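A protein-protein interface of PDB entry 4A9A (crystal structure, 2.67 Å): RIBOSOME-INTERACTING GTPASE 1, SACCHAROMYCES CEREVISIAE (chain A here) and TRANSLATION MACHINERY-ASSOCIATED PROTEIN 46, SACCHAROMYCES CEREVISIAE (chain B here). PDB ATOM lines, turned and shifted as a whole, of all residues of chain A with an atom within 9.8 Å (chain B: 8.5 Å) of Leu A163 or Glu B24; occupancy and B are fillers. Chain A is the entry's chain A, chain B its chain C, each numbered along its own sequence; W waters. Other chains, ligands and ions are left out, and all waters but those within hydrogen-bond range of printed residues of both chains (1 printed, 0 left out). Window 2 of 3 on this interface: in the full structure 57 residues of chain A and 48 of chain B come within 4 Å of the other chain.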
ATOM      1  N   PHE A  80       0.670   5.839 -26.775  1.00  0.00           N
ATOM      2  CA  PHE A  80       1.675   5.539 -27.789  1.00  0.00           C
ATOM      3  C   PHE A  80       2.090   4.075 -27.795  1.00  0.00           C
ATOM      4  O   PHE A  80       2.132   3.422 -26.752  1.00  0.00           O
ATOM      5  CB  PHE A  80       2.871   6.458 -27.644  1.00  0.00           C
ATOM      6  CG  PHE A  80       2.561   7.850 -28.044  1.00  0.00           C
ATOM      7  CD1 PHE A  80       1.770   8.660 -27.220  1.00  0.00           C
ATOM      8  CD2 PHE A  80       2.970   8.333 -29.281  1.00  0.00           C
ATOM      9  CE1 PHE A  80       1.455   9.944 -27.601  1.00  0.00           C
ATOM     10  CE2 PHE A  80       2.656   9.627 -29.674  1.00  0.00           C
ATOM     11  CZ  PHE A  80       1.900  10.434 -28.835  1.00  0.00           C
ATOM     12  N   ILE A 155      -5.525   6.516 -20.069  1.00  0.00           N
ATOM     13  CA  ILE A 155      -4.420   7.181 -20.728  1.00  0.00           C
ATOM     14  C   ILE A 155      -3.147   6.504 -20.257  1.00  0.00           C
ATOM     15  O   ILE A 155      -2.786   6.585 -19.069  1.00  0.00           O
ATOM     16  CB  ILE A 155      -4.427   8.653 -20.351  1.00  0.00           C
ATOM     17  CG1 ILE A 155      -5.704   9.260 -20.903  1.00  0.00           C
ATOM     18  CG2 ILE A 155      -3.180   9.377 -20.871  1.00  0.00           C
ATOM     19  CD1 ILE A 155      -5.862  10.718 -20.576  1.00  0.00           C
ATOM     20  N   ILE A 156      -2.477   5.814 -21.177  1.00  0.00           N
ATOM     21  CA  ILE A 156      -1.354   4.969 -20.808  1.00  0.00           C
ATOM     22  C   ILE A 156      -0.061   5.732 -20.939  1.00  0.00           C
ATOM     23  O   ILE A 156       0.297   6.181 -22.033  1.00  0.00           O
ATOM     24  CB  ILE A 156      -1.211   3.710 -21.692  1.00  0.00           C
ATOM     25  CG1 ILE A 156      -2.552   2.967 -21.949  1.00  0.00           C
ATOM     26  CG2 ILE A 156      -0.137   2.821 -21.105  1.00  0.00           C
ATOM     27  CD1 ILE A 156      -3.358   2.644 -20.703  1.00  0.00           C
ATOM     28  N   LEU A 157       0.660   5.859 -19.829  1.00  0.00           N
ATOM     29  CA  LEU A 157       1.946   6.543 -19.852  1.00  0.00           C
ATOM     30  C   LEU A 157       3.051   5.682 -19.308  1.00  0.00           C
ATOM     31  O   LEU A 157       2.809   4.742 -18.551  1.00  0.00           O
ATOM     32  CB  LEU A 157       1.868   7.851 -19.064  1.00  0.00           C
ATOM     33  CG  LEU A 157       0.679   8.714 -19.467  1.00  0.00           C
ATOM     34  CD1 LEU A 157       0.429   9.790 -18.418  1.00  0.00           C
ATOM     35  CD2 LEU A 157       0.901   9.287 -20.859  1.00  0.00           C
ATOM     36  N   ASP A 158       4.265   5.992 -19.727  1.00  0.00           N
ATOM     37  CA  ASP A 158       5.454   5.368 -19.188  1.00  0.00           C
ATOM     38  C   ASP A 158       5.984   6.399 -18.206  1.00  0.00           C
ATOM     39  O   ASP A 158       6.350   7.518 -18.583  1.00  0.00           O
ATOM     40  CB  ASP A 158       6.472   5.046 -20.301  1.00  0.00           C
ATOM     41  CG  ASP A 158       7.764   4.403 -19.768  1.00  0.00           C
ATOM     42  OD1 ASP A 158       8.258   4.789 -18.691  1.00  0.00           O
ATOM     43  OD2 ASP A 158       8.305   3.497 -20.436  1.00  0.00           O
ATOM     44  N   VAL A 159       6.011   6.021 -16.937  1.00  0.00           N
ATOM     45  CA  VAL A 159       6.313   6.968 -15.884  1.00  0.00           C
ATOM     46  C   VAL A 159       7.753   7.458 -15.988  1.00  0.00           C
ATOM     47  O   VAL A 159       8.118   8.413 -15.325  1.00  0.00           O
ATOM     48  CB  VAL A 159       5.992   6.381 -14.485  1.00  0.00           C
ATOM     49  CG1 VAL A 159       7.036   5.367 -14.042  1.00  0.00           C
ATOM     50  CG2 VAL A 159       5.857   7.488 -13.458  1.00  0.00           C
ATOM     51  N   ASN A 160       8.570   6.816 -16.817  1.00  0.00           N
ATOM     52  CA  ASN A 160       9.901   7.341 -17.066  1.00  0.00           C
ATOM     53  C   ASN A 160       9.963   8.483 -18.079  1.00  0.00           C
ATOM     54  O   ASN A 160      11.003   9.139 -18.203  1.00  0.00           O
ATOM     55  CB  ASN A 160      10.847   6.236 -17.488  1.00  0.00           C
ATOM     56  CG  ASN A 160      11.043   5.204 -16.408  1.00  0.00           C
ATOM     57  OD1 ASN A 160      10.797   4.021 -16.624  1.00  0.00           O
ATOM     58  ND2 ASN A 160      11.489   5.640 -15.241  1.00  0.00           N
ATOM     59  N   LYS A 161       8.865   8.718 -18.799  1.00  0.00           N
ATOM     60  CA  LYS A 161       8.796   9.770 -19.814  1.00  0.00           C
ATOM     61  C   LYS A 161       7.353  10.226 -20.050  1.00  0.00           C
ATOM     62  O   LYS A 161       6.881  10.263 -21.187  1.00  0.00           O
ATOM     63  CB  LYS A 161       9.439   9.293 -21.127  1.00  0.00           C
ATOM     64  CG  LYS A 161       8.922   7.951 -21.638  1.00  0.00           C
ATOM     65  CD  LYS A 161       9.451   7.612 -23.024  1.00  0.00           C
ATOM     66  CE  LYS A 161       8.649   6.457 -23.610  1.00  0.00           C
ATOM     67  NZ  LYS A 161       9.431   5.658 -24.588  1.00  0.00           N
ATOM     68  N   PRO A 162       6.639  10.581 -18.981  1.00  0.00           N
ATOM     69  CA  PRO A 162       5.209  10.829 -19.142  1.00  0.00           C
ATOM     70  C   PRO A 162       4.800  12.119 -19.857  1.00  0.00           C
ATOM     71  O   PRO A 162       3.745  12.129 -20.495  1.00  0.00           O
ATOM     72  CB  PRO A 162       4.706  10.893 -17.699  1.00  0.00           C
ATOM     73  CG  PRO A 162       5.888  11.344 -16.911  1.00  0.00           C
ATOM     74  CD  PRO A 162       7.071  10.702 -17.576  1.00  0.00           C
ATOM     75  N   LEU A 163       5.584  13.195 -19.749  1.00  0.00           N
ATOM     76  CA  LEU A 163       5.036  14.533 -20.046  1.00  0.00           C
ATOM     77  C   LEU A 163       4.764  14.799 -21.502  1.00  0.00           C
ATOM     78  O   LEU A 163       3.662  15.218 -21.861  1.00  0.00           O
ATOM     79  CB  LEU A 163       5.853  15.664 -19.415  1.00  0.00           C
ATOM     80  CG  LEU A 163       6.022  15.544 -17.888  1.00  0.00           C
ATOM     81  CD1 LEU A 163       6.736  16.756 -17.323  1.00  0.00           C
ATOM     82  CD2 LEU A 163       4.699  15.275 -17.152  1.00  0.00           C
ATOM     83  N   HIS A 164       5.744  14.531 -22.354  1.00  0.00           N
ATOM     84  CA  HIS A 164       5.540  14.754 -23.778  1.00  0.00           C
ATOM     85  C   HIS A 164       4.293  14.047 -24.239  1.00  0.00           C
ATOM     86  O   HIS A 164       3.404  14.678 -24.802  1.00  0.00           O
ATOM     87  CB  HIS A 164       6.756  14.334 -24.582  1.00  0.00           C
ATOM     88  CG  HIS A 164       6.573  14.476 -26.069  1.00  0.00           C
ATOM     89  ND1 HIS A 164       6.665  15.668 -26.704  1.00  0.00           N
ATOM     90  CD2 HIS A 164       6.285  13.523 -27.053  1.00  0.00           C
ATOM     91  CE1 HIS A 164       6.443  15.492 -28.025  1.00  0.00           C
ATOM     92  NE2 HIS A 164       6.208  14.178 -28.237  1.00  0.00           N
ATOM     93  N   HIS A 165       4.187  12.746 -23.965  1.00  0.00           N
ATOM     94  CA  HIS A 165       3.037  11.970 -24.427  1.00  0.00           C
ATOM     95  C   HIS A 165       1.718  12.408 -23.857  1.00  0.00           C
ATOM     96  O   HIS A 165       0.715  12.424 -24.568  1.00  0.00           O
ATOM     97  CB  HIS A 165       3.257  10.482 -24.212  1.00  0.00           C
ATOM     98  CG  HIS A 165       4.227   9.877 -25.202  1.00  0.00           C
ATOM     99  ND1 HIS A 165       4.987   8.804 -24.919  1.00  0.00           N
ATOM    100  CD2 HIS A 165       4.565  10.264 -26.508  1.00  0.00           C
ATOM    101  CE1 HIS A 165       5.757   8.501 -25.984  1.00  0.00           C
ATOM    102  NE2 HIS A 165       5.493   9.388 -26.960  1.00  0.00           N
ATOM    103  N   LYS A 166       1.713  12.782 -22.580  1.00  0.00           N
ATOM    104  CA  LYS A 166       0.505  13.201 -21.901  1.00  0.00           C
ATOM    105  C   LYS A 166      -0.030  14.462 -22.549  1.00  0.00           C
ATOM    106  O   LYS A 166      -1.231  14.613 -22.790  1.00  0.00           O
ATOM    107  CB  LYS A 166       0.815  13.426 -20.424  1.00  0.00           C
ATOM    108  CG  LYS A 166      -0.173  14.286 -19.660  1.00  0.00           C
ATOM    109  CD  LYS A 166      -0.307  13.784 -18.232  1.00  0.00           C
ATOM    110  CE  LYS A 166      -0.628  14.890 -17.236  1.00  0.00           C
ATOM    111  NZ  LYS A 166      -1.690  15.837 -17.694  1.00  0.00           N
ATOM    112  N   GLN A 167       0.884  15.356 -22.867  1.00  0.00           N
ATOM    113  CA  GLN A 167       0.519  16.632 -23.422  1.00  0.00           C
ATOM    114  C   GLN A 167      -0.166  16.471 -24.778  1.00  0.00           C
ATOM    115  O   GLN A 167      -1.157  17.151 -25.040  1.00  0.00           O
ATOM    116  CB  GLN A 167       1.756  17.498 -23.530  1.00  0.00           C
ATOM    117  CG  GLN A 167       1.463  18.959 -23.741  1.00  0.00           C
ATOM    118  CD  GLN A 167       2.321  19.542 -24.845  1.00  0.00           C
ATOM    119  OE1 GLN A 167       2.183  19.160 -26.016  1.00  0.00           O
ATOM    120  NE2 GLN A 167       3.213  20.473 -24.487  1.00  0.00           N
ATOM    121  N   ILE A 168       0.343  15.566 -25.620  1.00  0.00           N
ATOM    122  CA  ILE A 168      -0.245  15.300 -26.943  1.00  0.00           C
ATOM    123  C   ILE A 168      -1.625  14.641 -26.804  1.00  0.00           C
ATOM    124  O   ILE A 168      -2.599  15.019 -27.479  1.00  0.00           O
ATOM    125  CB  ILE A 168       0.649  14.401 -27.847  1.00  0.00           C
ATOM    126  CG1 ILE A 168       2.104  14.906 -27.954  1.00  0.00           C
ATOM    127  CG2 ILE A 168       0.053  14.267 -29.232  1.00  0.00           C
ATOM    128  CD1 ILE A 168       2.279  16.256 -28.622  1.00  0.00           C
ATOM    129  N   ILE A 169      -1.714  13.660 -25.925  1.00  0.00           N
ATOM    130  CA  ILE A 169      -2.945  12.922 -25.763  1.00  0.00           C
ATOM    131  C   ILE A 169      -4.056  13.887 -25.310  1.00  0.00           C
ATOM    132  O   ILE A 169      -5.161  13.923 -25.872  1.00  0.00           O
ATOM    133  CB  ILE A 169      -2.728  11.748 -24.801  1.00  0.00           C
ATOM    134  CG1 ILE A 169      -1.863  10.680 -25.476  1.00  0.00           C
ATOM    135  CG2 ILE A 169      -4.050  11.142 -24.382  1.00  0.00           C
ATOM    136  CD1 ILE A 169      -1.333   9.631 -24.519  1.00  0.00           C
ATOM    137  N   GLU A 170      -3.737  14.700 -24.315  1.00  0.00           N
ATOM    138  CA  GLU A 170      -4.694  15.664 -23.822  1.00  0.00           C
ATOM    139  C   GLU A 170      -5.086  16.648 -24.902  1.00  0.00           C
ATOM    140  O   GLU A 170      -6.258  16.803 -25.157  1.00  0.00           O
ATOM    141  CB  GLU A 170      -4.193  16.327 -22.546  1.00  0.00           C
ATOM    142  CG  GLU A 170      -4.208  15.315 -21.428  1.00  0.00           C
ATOM    143  CD  GLU A 170      -3.691  15.817 -20.108  1.00  0.00           C
ATOM    144  OE1 GLU A 170      -2.899  16.785 -20.065  1.00  0.00           O
ATOM    145  OE2 GLU A 170      -4.068  15.198 -19.092  1.00  0.00           O
ATOM    146  N   LYS A 171      -4.123  17.256 -25.584  1.00  0.00           N
ATOM    147  CA  LYS A 171      -4.461  18.200 -26.657  1.00  0.00           C
ATOM    148  C   LYS A 171      -5.443  17.584 -27.668  1.00  0.00           C
ATOM    149  O   LYS A 171      -6.433  18.211 -28.031  1.00  0.00           O
ATOM    150  CB  LYS A 171      -3.206  18.741 -27.345  1.00  0.00           C
ATOM    151  CG  LYS A 171      -3.451  19.402 -28.690  1.00  0.00           C
ATOM    152  CD  LYS A 171      -2.168  20.007 -29.242  1.00  0.00           C
ATOM    153  CE  LYS A 171      -2.347  20.527 -30.669  1.00  0.00           C
ATOM    154  NZ  LYS A 171      -3.317  21.657 -30.803  1.00  0.00           N
ATOM    155  N   TYR A 254      -5.218   7.882 -15.457  1.00  0.00           N
ATOM    156  CA  TYR A 254      -3.836   7.956 -15.904  1.00  0.00           C
ATOM    157  C   TYR A 254      -3.099   6.724 -15.427  1.00  0.00           C
ATOM    158  O   TYR A 254      -2.854   6.553 -14.233  1.00  0.00           O
ATOM    159  CB  TYR A 254      -3.172   9.227 -15.405  1.00  0.00           C
ATOM    160  CG  TYR A 254      -3.801  10.451 -16.020  1.00  0.00           C
ATOM    161  CD1 TYR A 254      -3.365  10.943 -17.248  1.00  0.00           C
ATOM    162  CD2 TYR A 254      -4.858  11.095 -15.393  1.00  0.00           C
ATOM    163  CE1 TYR A 254      -3.962  12.045 -17.826  1.00  0.00           C
ATOM    164  CE2 TYR A 254      -5.460  12.193 -15.962  1.00  0.00           C
ATOM    165  CZ  TYR A 254      -5.013  12.665 -17.171  1.00  0.00           C
ATOM    166  OH  TYR A 254      -5.624  13.775 -17.711  1.00  0.00           O
ATOM    167  N   LEU A 256       0.060   4.756 -15.058  1.00  0.00           N
ATOM    168  CA  LEU A 256       1.482   5.078 -15.095  1.00  0.00           C
ATOM    169  C   LEU A 256       2.296   3.799 -15.017  1.00  0.00           C
ATOM    170  O   LEU A 256       2.563   3.272 -13.929  1.00  0.00           O
ATOM    171  CB  LEU A 256       1.844   6.053 -13.967  1.00  0.00           C
ATOM    172  CG  LEU A 256       0.868   7.220 -13.771  1.00  0.00           C
ATOM    173  CD1 LEU A 256       1.166   8.029 -12.527  1.00  0.00           C
ATOM    174  CD2 LEU A 256       0.837   8.120 -14.999  1.00  0.00           C
ATOM    175  N   LEU A 269       4.511   8.368  -3.606  1.00  0.00           N
ATOM    176  CA  LEU A 269       4.339   9.722  -4.095  1.00  0.00           C
ATOM    177  C   LEU A 269       3.373   9.866  -5.300  1.00  0.00           C
ATOM    178  O   LEU A 269       2.668  10.872  -5.422  1.00  0.00           O
ATOM    179  CB  LEU A 269       5.717  10.249  -4.448  1.00  0.00           C
ATOM    180  CG  LEU A 269       5.955  11.734  -4.653  1.00  0.00           C
ATOM    181  CD1 LEU A 269       5.537  12.508  -3.416  1.00  0.00           C
ATOM    182  CD2 LEU A 269       7.438  11.933  -4.967  1.00  0.00           C
ATOM    183  N   ILE A 273      -1.173  12.151  -6.960  1.00  0.00           N
ATOM    184  CA  ILE A 273      -1.690  12.647  -8.227  1.00  0.00           C
ATOM    185  C   ILE A 273      -3.081  12.078  -8.432  1.00  0.00           C
ATOM    186  O   ILE A 273      -3.229  10.868  -8.506  1.00  0.00           O
ATOM    187  CB  ILE A 273      -0.828  12.188  -9.423  1.00  0.00           C
ATOM    188  CG1 ILE A 273       0.629  12.642  -9.278  1.00  0.00           C
ATOM    189  CG2 ILE A 273      -1.409  12.694 -10.737  1.00  0.00           C
ATOM    190  CD1 ILE A 273       1.593  11.753 -10.037  1.00  0.00           C
ATOM    191  N   THR B  18       0.503  17.475  -9.368  1.00  0.00           N
ATOM    192  CA  THR B  18       0.350  17.034 -10.754  1.00  0.00           C
ATOM    193  C   THR B  18       1.495  16.108 -11.112  1.00  0.00           C
ATOM    194  O   THR B  18       2.515  16.047 -10.429  1.00  0.00           O
ATOM    195  CB  THR B  18       0.351  18.202 -11.756  1.00  0.00           C
ATOM    196  OG1 THR B  18       1.537  18.989 -11.568  1.00  0.00           O
ATOM    197  CG2 THR B  18      -0.893  19.058 -11.595  1.00  0.00           C
ATOM    198  N   LEU B  19       1.317  15.388 -12.202  1.00  0.00           N
ATOM    199  CA  LEU B  19       2.369  14.564 -12.761  1.00  0.00           C
ATOM    200  C   LEU B  19       3.542  15.450 -13.204  1.00  0.00           C
ATOM    201  O   LEU B  19       4.696  15.042 -13.136  1.00  0.00           O
ATOM    202  CB  LEU B  19       1.781  13.788 -13.928  1.00  0.00           C
ATOM    203  CG  LEU B  19       2.532  12.689 -14.655  1.00  0.00           C
ATOM    204  CD1 LEU B  19       3.119  11.664 -13.696  1.00  0.00           C
ATOM    205  CD2 LEU B  19       1.575  12.042 -15.634  1.00  0.00           C
ATOM    206  N   GLU B  20       3.233  16.670 -13.635  1.00  0.00           N
ATOM    207  CA  GLU B  20       4.251  17.656 -13.996  1.00  0.00           C
ATOM    208  C   GLU B  20       5.059  18.014 -12.757  1.00  0.00           C
ATOM    209  O   GLU B  20       6.294  17.965 -12.780  1.00  0.00           O
ATOM    210  CB  GLU B  20       3.624  18.921 -14.612  1.00  0.00           C
ATOM    211  CG  GLU B  20       2.970  18.752 -15.987  1.00  0.00           C
ATOM    212  CD  GLU B  20       1.662  17.940 -15.979  1.00  0.00           C
ATOM    213  OE1 GLU B  20       1.094  17.688 -14.888  1.00  0.00           O
ATOM    214  OE2 GLU B  20       1.190  17.537 -17.074  1.00  0.00           O
ATOM    215  N   GLU B  21       4.357  18.358 -11.678  1.00  0.00           N
ATOM    216  CA  GLU B  21       5.009  18.713 -10.422  1.00  0.00           C
ATOM    217  C   GLU B  21       5.884  17.565  -9.925  1.00  0.00           C
ATOM    218  O   GLU B  21       7.002  17.788  -9.424  1.00  0.00           O
ATOM    219  CB  GLU B  21       3.974  19.067  -9.365  1.00  0.00           C
ATOM    220  CG  GLU B  21       3.539  20.517  -9.360  1.00  0.00           C
ATOM    221  CD  GLU B  21       2.166  20.696  -8.733  1.00  0.00           C
ATOM    222  OE1 GLU B  21       1.231  19.984  -9.120  1.00  0.00           O
ATOM    223  OE2 GLU B  21       2.007  21.554  -7.858  1.00  0.00           O
ATOM    224  N   PHE B  22       5.373  16.343 -10.081  1.00  0.00           N
ATOM    225  CA  PHE B  22       6.097  15.131  -9.701  1.00  0.00           C
ATOM    226  C   PHE B  22       7.413  15.008 -10.443  1.00  0.00           C
ATOM    227  O   PHE B  22       8.445  14.763  -9.832  1.00  0.00           O
ATOM    228  CB  PHE B  22       5.253  13.882  -9.961  1.00  0.00           C
ATOM    229  CG  PHE B  22       6.032  12.600  -9.877  1.00  0.00           C
ATOM    230  CD1 PHE B  22       6.242  11.976  -8.652  1.00  0.00           C
ATOM    231  CD2 PHE B  22       6.567  12.016 -11.025  1.00  0.00           C
ATOM    232  CE1 PHE B  22       6.966  10.794  -8.577  1.00  0.00           C
ATOM    233  CE2 PHE B  22       7.295  10.838 -10.960  1.00  0.00           C
ATOM    234  CZ  PHE B  22       7.493  10.225  -9.737  1.00  0.00           C
ATOM    235  N   ILE B  23       7.362  15.161 -11.761  1.00  0.00           N
ATOM    236  CA  ILE B  23       8.541  15.020 -12.601  1.00  0.00           C
ATOM    237  C   ILE B  23       9.521  16.157 -12.359  1.00  0.00           C
ATOM    238  O   ILE B  23      10.730  15.942 -12.278  1.00  0.00           O
ATOM    239  CB  ILE B  23       8.160  14.958 -14.098  1.00  0.00           C
ATOM    240  CG1 ILE B  23       7.413  13.647 -14.409  1.00  0.00           C
ATOM    241  CG2 ILE B  23       9.375  15.132 -15.001  1.00  0.00           C
ATOM    242  CD1 ILE B  23       8.258  12.388 -14.357  1.00  0.00           C
ATOM    243  N   GLU B  24       8.998  17.361 -12.215  1.00  0.00           N
ATOM    244  CA  GLU B  24       9.852  18.520 -12.267  1.00  0.00           C
ATOM    245  C   GLU B  24      10.469  18.907 -10.933  1.00  0.00           C
ATOM    246  O   GLU B  24      11.572  19.446 -10.903  1.00  0.00           O
ATOM    247  CB  GLU B  24       9.127  19.693 -12.932  1.00  0.00           C
ATOM    248  CG  GLU B  24       9.163  19.596 -14.454  1.00  0.00           C
ATOM    249  CD  GLU B  24       8.051  20.365 -15.159  1.00  0.00           C
ATOM    250  OE1 GLU B  24       7.640  21.460 -14.691  1.00  0.00           O
ATOM    251  OE2 GLU B  24       7.592  19.866 -16.211  1.00  0.00           O
ATOM    252  N   THR B  25       9.780  18.628  -9.830  1.00  0.00           N
ATOM    253  CA  THR B  25      10.266  19.089  -8.521  1.00  0.00           C
ATOM    254  C   THR B  25      10.132  18.066  -7.390  1.00  0.00           C
ATOM    255  O   THR B  25      11.021  17.958  -6.551  1.00  0.00           O
ATOM    256  CB  THR B  25       9.598  20.415  -8.076  1.00  0.00           C
ATOM    257  OG1 THR B  25       8.180  20.243  -8.037  1.00  0.00           O
ATOM    258  CG2 THR B  25       9.929  21.564  -9.026  1.00  0.00           C
ATOM    259  N   GLU B  26       9.027  17.325  -7.361  1.00  0.00           N
ATOM    260  CA  GLU B  26       8.714  16.511  -6.186  1.00  0.00           C
ATOM    261  C   GLU B  26       9.620  15.304  -6.026  1.00  0.00           C
ATOM    262  O   GLU B  26      10.135  15.039  -4.943  1.00  0.00           O
ATOM    263  CB  GLU B  26       7.244  16.105  -6.164  1.00  0.00           C
ATOM    264  CG  GLU B  26       6.282  17.259  -5.887  1.00  0.00           C
ATOM    265  CD  GLU B  26       6.520  17.976  -4.562  1.00  0.00           C
ATOM    266  OE1 GLU B  26       6.995  17.355  -3.587  1.00  0.00           O
ATOM    267  OE2 GLU B  26       6.230  19.186  -4.489  1.00  0.00           O
ATOM    268  N   ARG B  27       9.828  14.600  -7.124  1.00  0.00           N
ATOM    269  CA  ARG B  27      10.693  13.446  -7.177  1.00  0.00           C
ATOM    270  C   ARG B  27      12.108  13.778  -6.721  1.00  0.00           C
ATOM    271  O   ARG B  27      12.794  12.932  -6.145  1.00  0.00           O
ATOM    272  CB  ARG B  27      10.740  12.952  -8.604  1.00  0.00           C
ATOM    273  CG  ARG B  27      11.081  11.495  -8.720  1.00  0.00           C
ATOM    274  CD  ARG B  27      11.490  11.149 -10.131  1.00  0.00           C
ATOM    275  NE  ARG B  27      12.083   9.826 -10.123  1.00  0.00           N
ATOM    276  CZ  ARG B  27      12.765   9.299 -11.126  1.00  0.00           C
ATOM    277  NH1 ARG B  27      12.946   9.976 -12.249  1.00  0.00           N
ATOM    278  NH2 ARG B  27      13.252   8.074 -11.005  1.00  0.00           N
ATOM    279  N   GLY B  28      12.539  15.012  -6.967  1.00  0.00           N
ATOM    280  CA  GLY B  28      13.901  15.418  -6.650  1.00  0.00           C
ATOM    281  C   GLY B  28      14.120  15.835  -5.209  1.00  0.00           C
ATOM    282  O   GLY B  28      15.266  15.991  -4.777  1.00  0.00           O
ATOM    283  N   LYS B  29      13.032  16.030  -4.464  1.00  0.00           N
ATOM    284  CA  LYS B  29      13.134  16.386  -3.045  1.00  0.00           C
ATOM    285  C   LYS B  29      13.636  15.188  -2.234  1.00  0.00           C
ATOM    286  O   LYS B  29      14.176  15.348  -1.137  1.00  0.00           O
ATOM    287  CB  LYS B  29      11.792  16.871  -2.483  1.00  0.00           C
ATOM    288  CG  LYS B  29      11.216  18.108  -3.148  1.00  0.00           C
ATOM    289  CD  LYS B  29      10.177  18.759  -2.246  1.00  0.00           C
ATOM    290  CE  LYS B  29       9.255  19.708  -3.003  1.00  0.00           C
ATOM    291  NZ  LYS B  29       8.481  20.596  -2.089  1.00  0.00           N
HETATM  292  O   HOH W   1      12.314   7.764 -14.130  1.00  0.00           O
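OE2 of Glu B20 lies within salt-bridge range of NZ of Lys A166, at 3.4 Å.
OE1 of Glu A170 lies within salt-bridge range of NZ of Lys A166 (2.8 Å).
The backbone carbonyl oxygen (O) of Phe B22 is in hydrogen-bond range of the backbone NH (N) of Arg B27.
Leu B19 touches Leu A157 (CD2 to CD1, 3.8 Å).
Pro A162 touches Leu B19 (CB to CD2, 3.9 Å).
Ile B23 touches Pro A162.
CA of Glu B20 touches CD2 of Leu A163, 3.98 Å away.
CG2 of Ile B23 touches CD1 of Leu A163, at 3.9 Å.
Leu A163 touches Glu B24 (CD1 to OE2, 3.4 Å).
Lys A166 touches Leu B19.
CE1 of Phe B22 touches CD2 of Leu A269, at 3.8 Å.
Ile A273 touches Leu B19 (CD1 to CD1, 3.97 Å).
Of the printed residues of chain A, Glu B24 touches Leu A163.
Pro A162 touches just these residues of chain B: Leu B19 and Ile B23.
Glu B20 touches two residues of chain A.
Ile B23 touches two residues of chain A.
Of the printed residues of chain B, Ile A273 touches Leu B19 (3.97 Å).
Printed residues of chain B within 4 Å of Lys A166: Leu B19 and Glu B20.
Printed residues of chain A within 4 Å of Phe B22: Leu A269 (3.8 Å).
The nearest residue of chain B that does not touch Leu A163 is Leu B19 (4.02 Å).
The nearest printed residue of chain B that does not touch Leu A157 is Glu B20 (7.9 Å).
Printed residues of chain B that touch a printed residue of chain A: Leu B19, Glu B20, Phe B22, Ile B23 and Glu B24.
Hydrophobic or aromatic side chains of chain B that line the printed part of chain A: Leu B19, Phe B22 and Ile B23.
Of the 22 printed residues of chain A, 6 touch a printed residue of chain B.
Among the printed residues, 10 pairs touch across the chains.
Among the printed residues, Asp or Glu carboxylates within 4 Å of a Lys or Arg side-chain nitrogen of the other chain: Lys A166 with Glu B20.
Water W1 lies within hydrogen-bond range of the side-chain amide nitrogen (ND2) of Asn A160 (2.5 Å) and the guanidinium group (NH1) of Arg B27 (3.0 Å).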
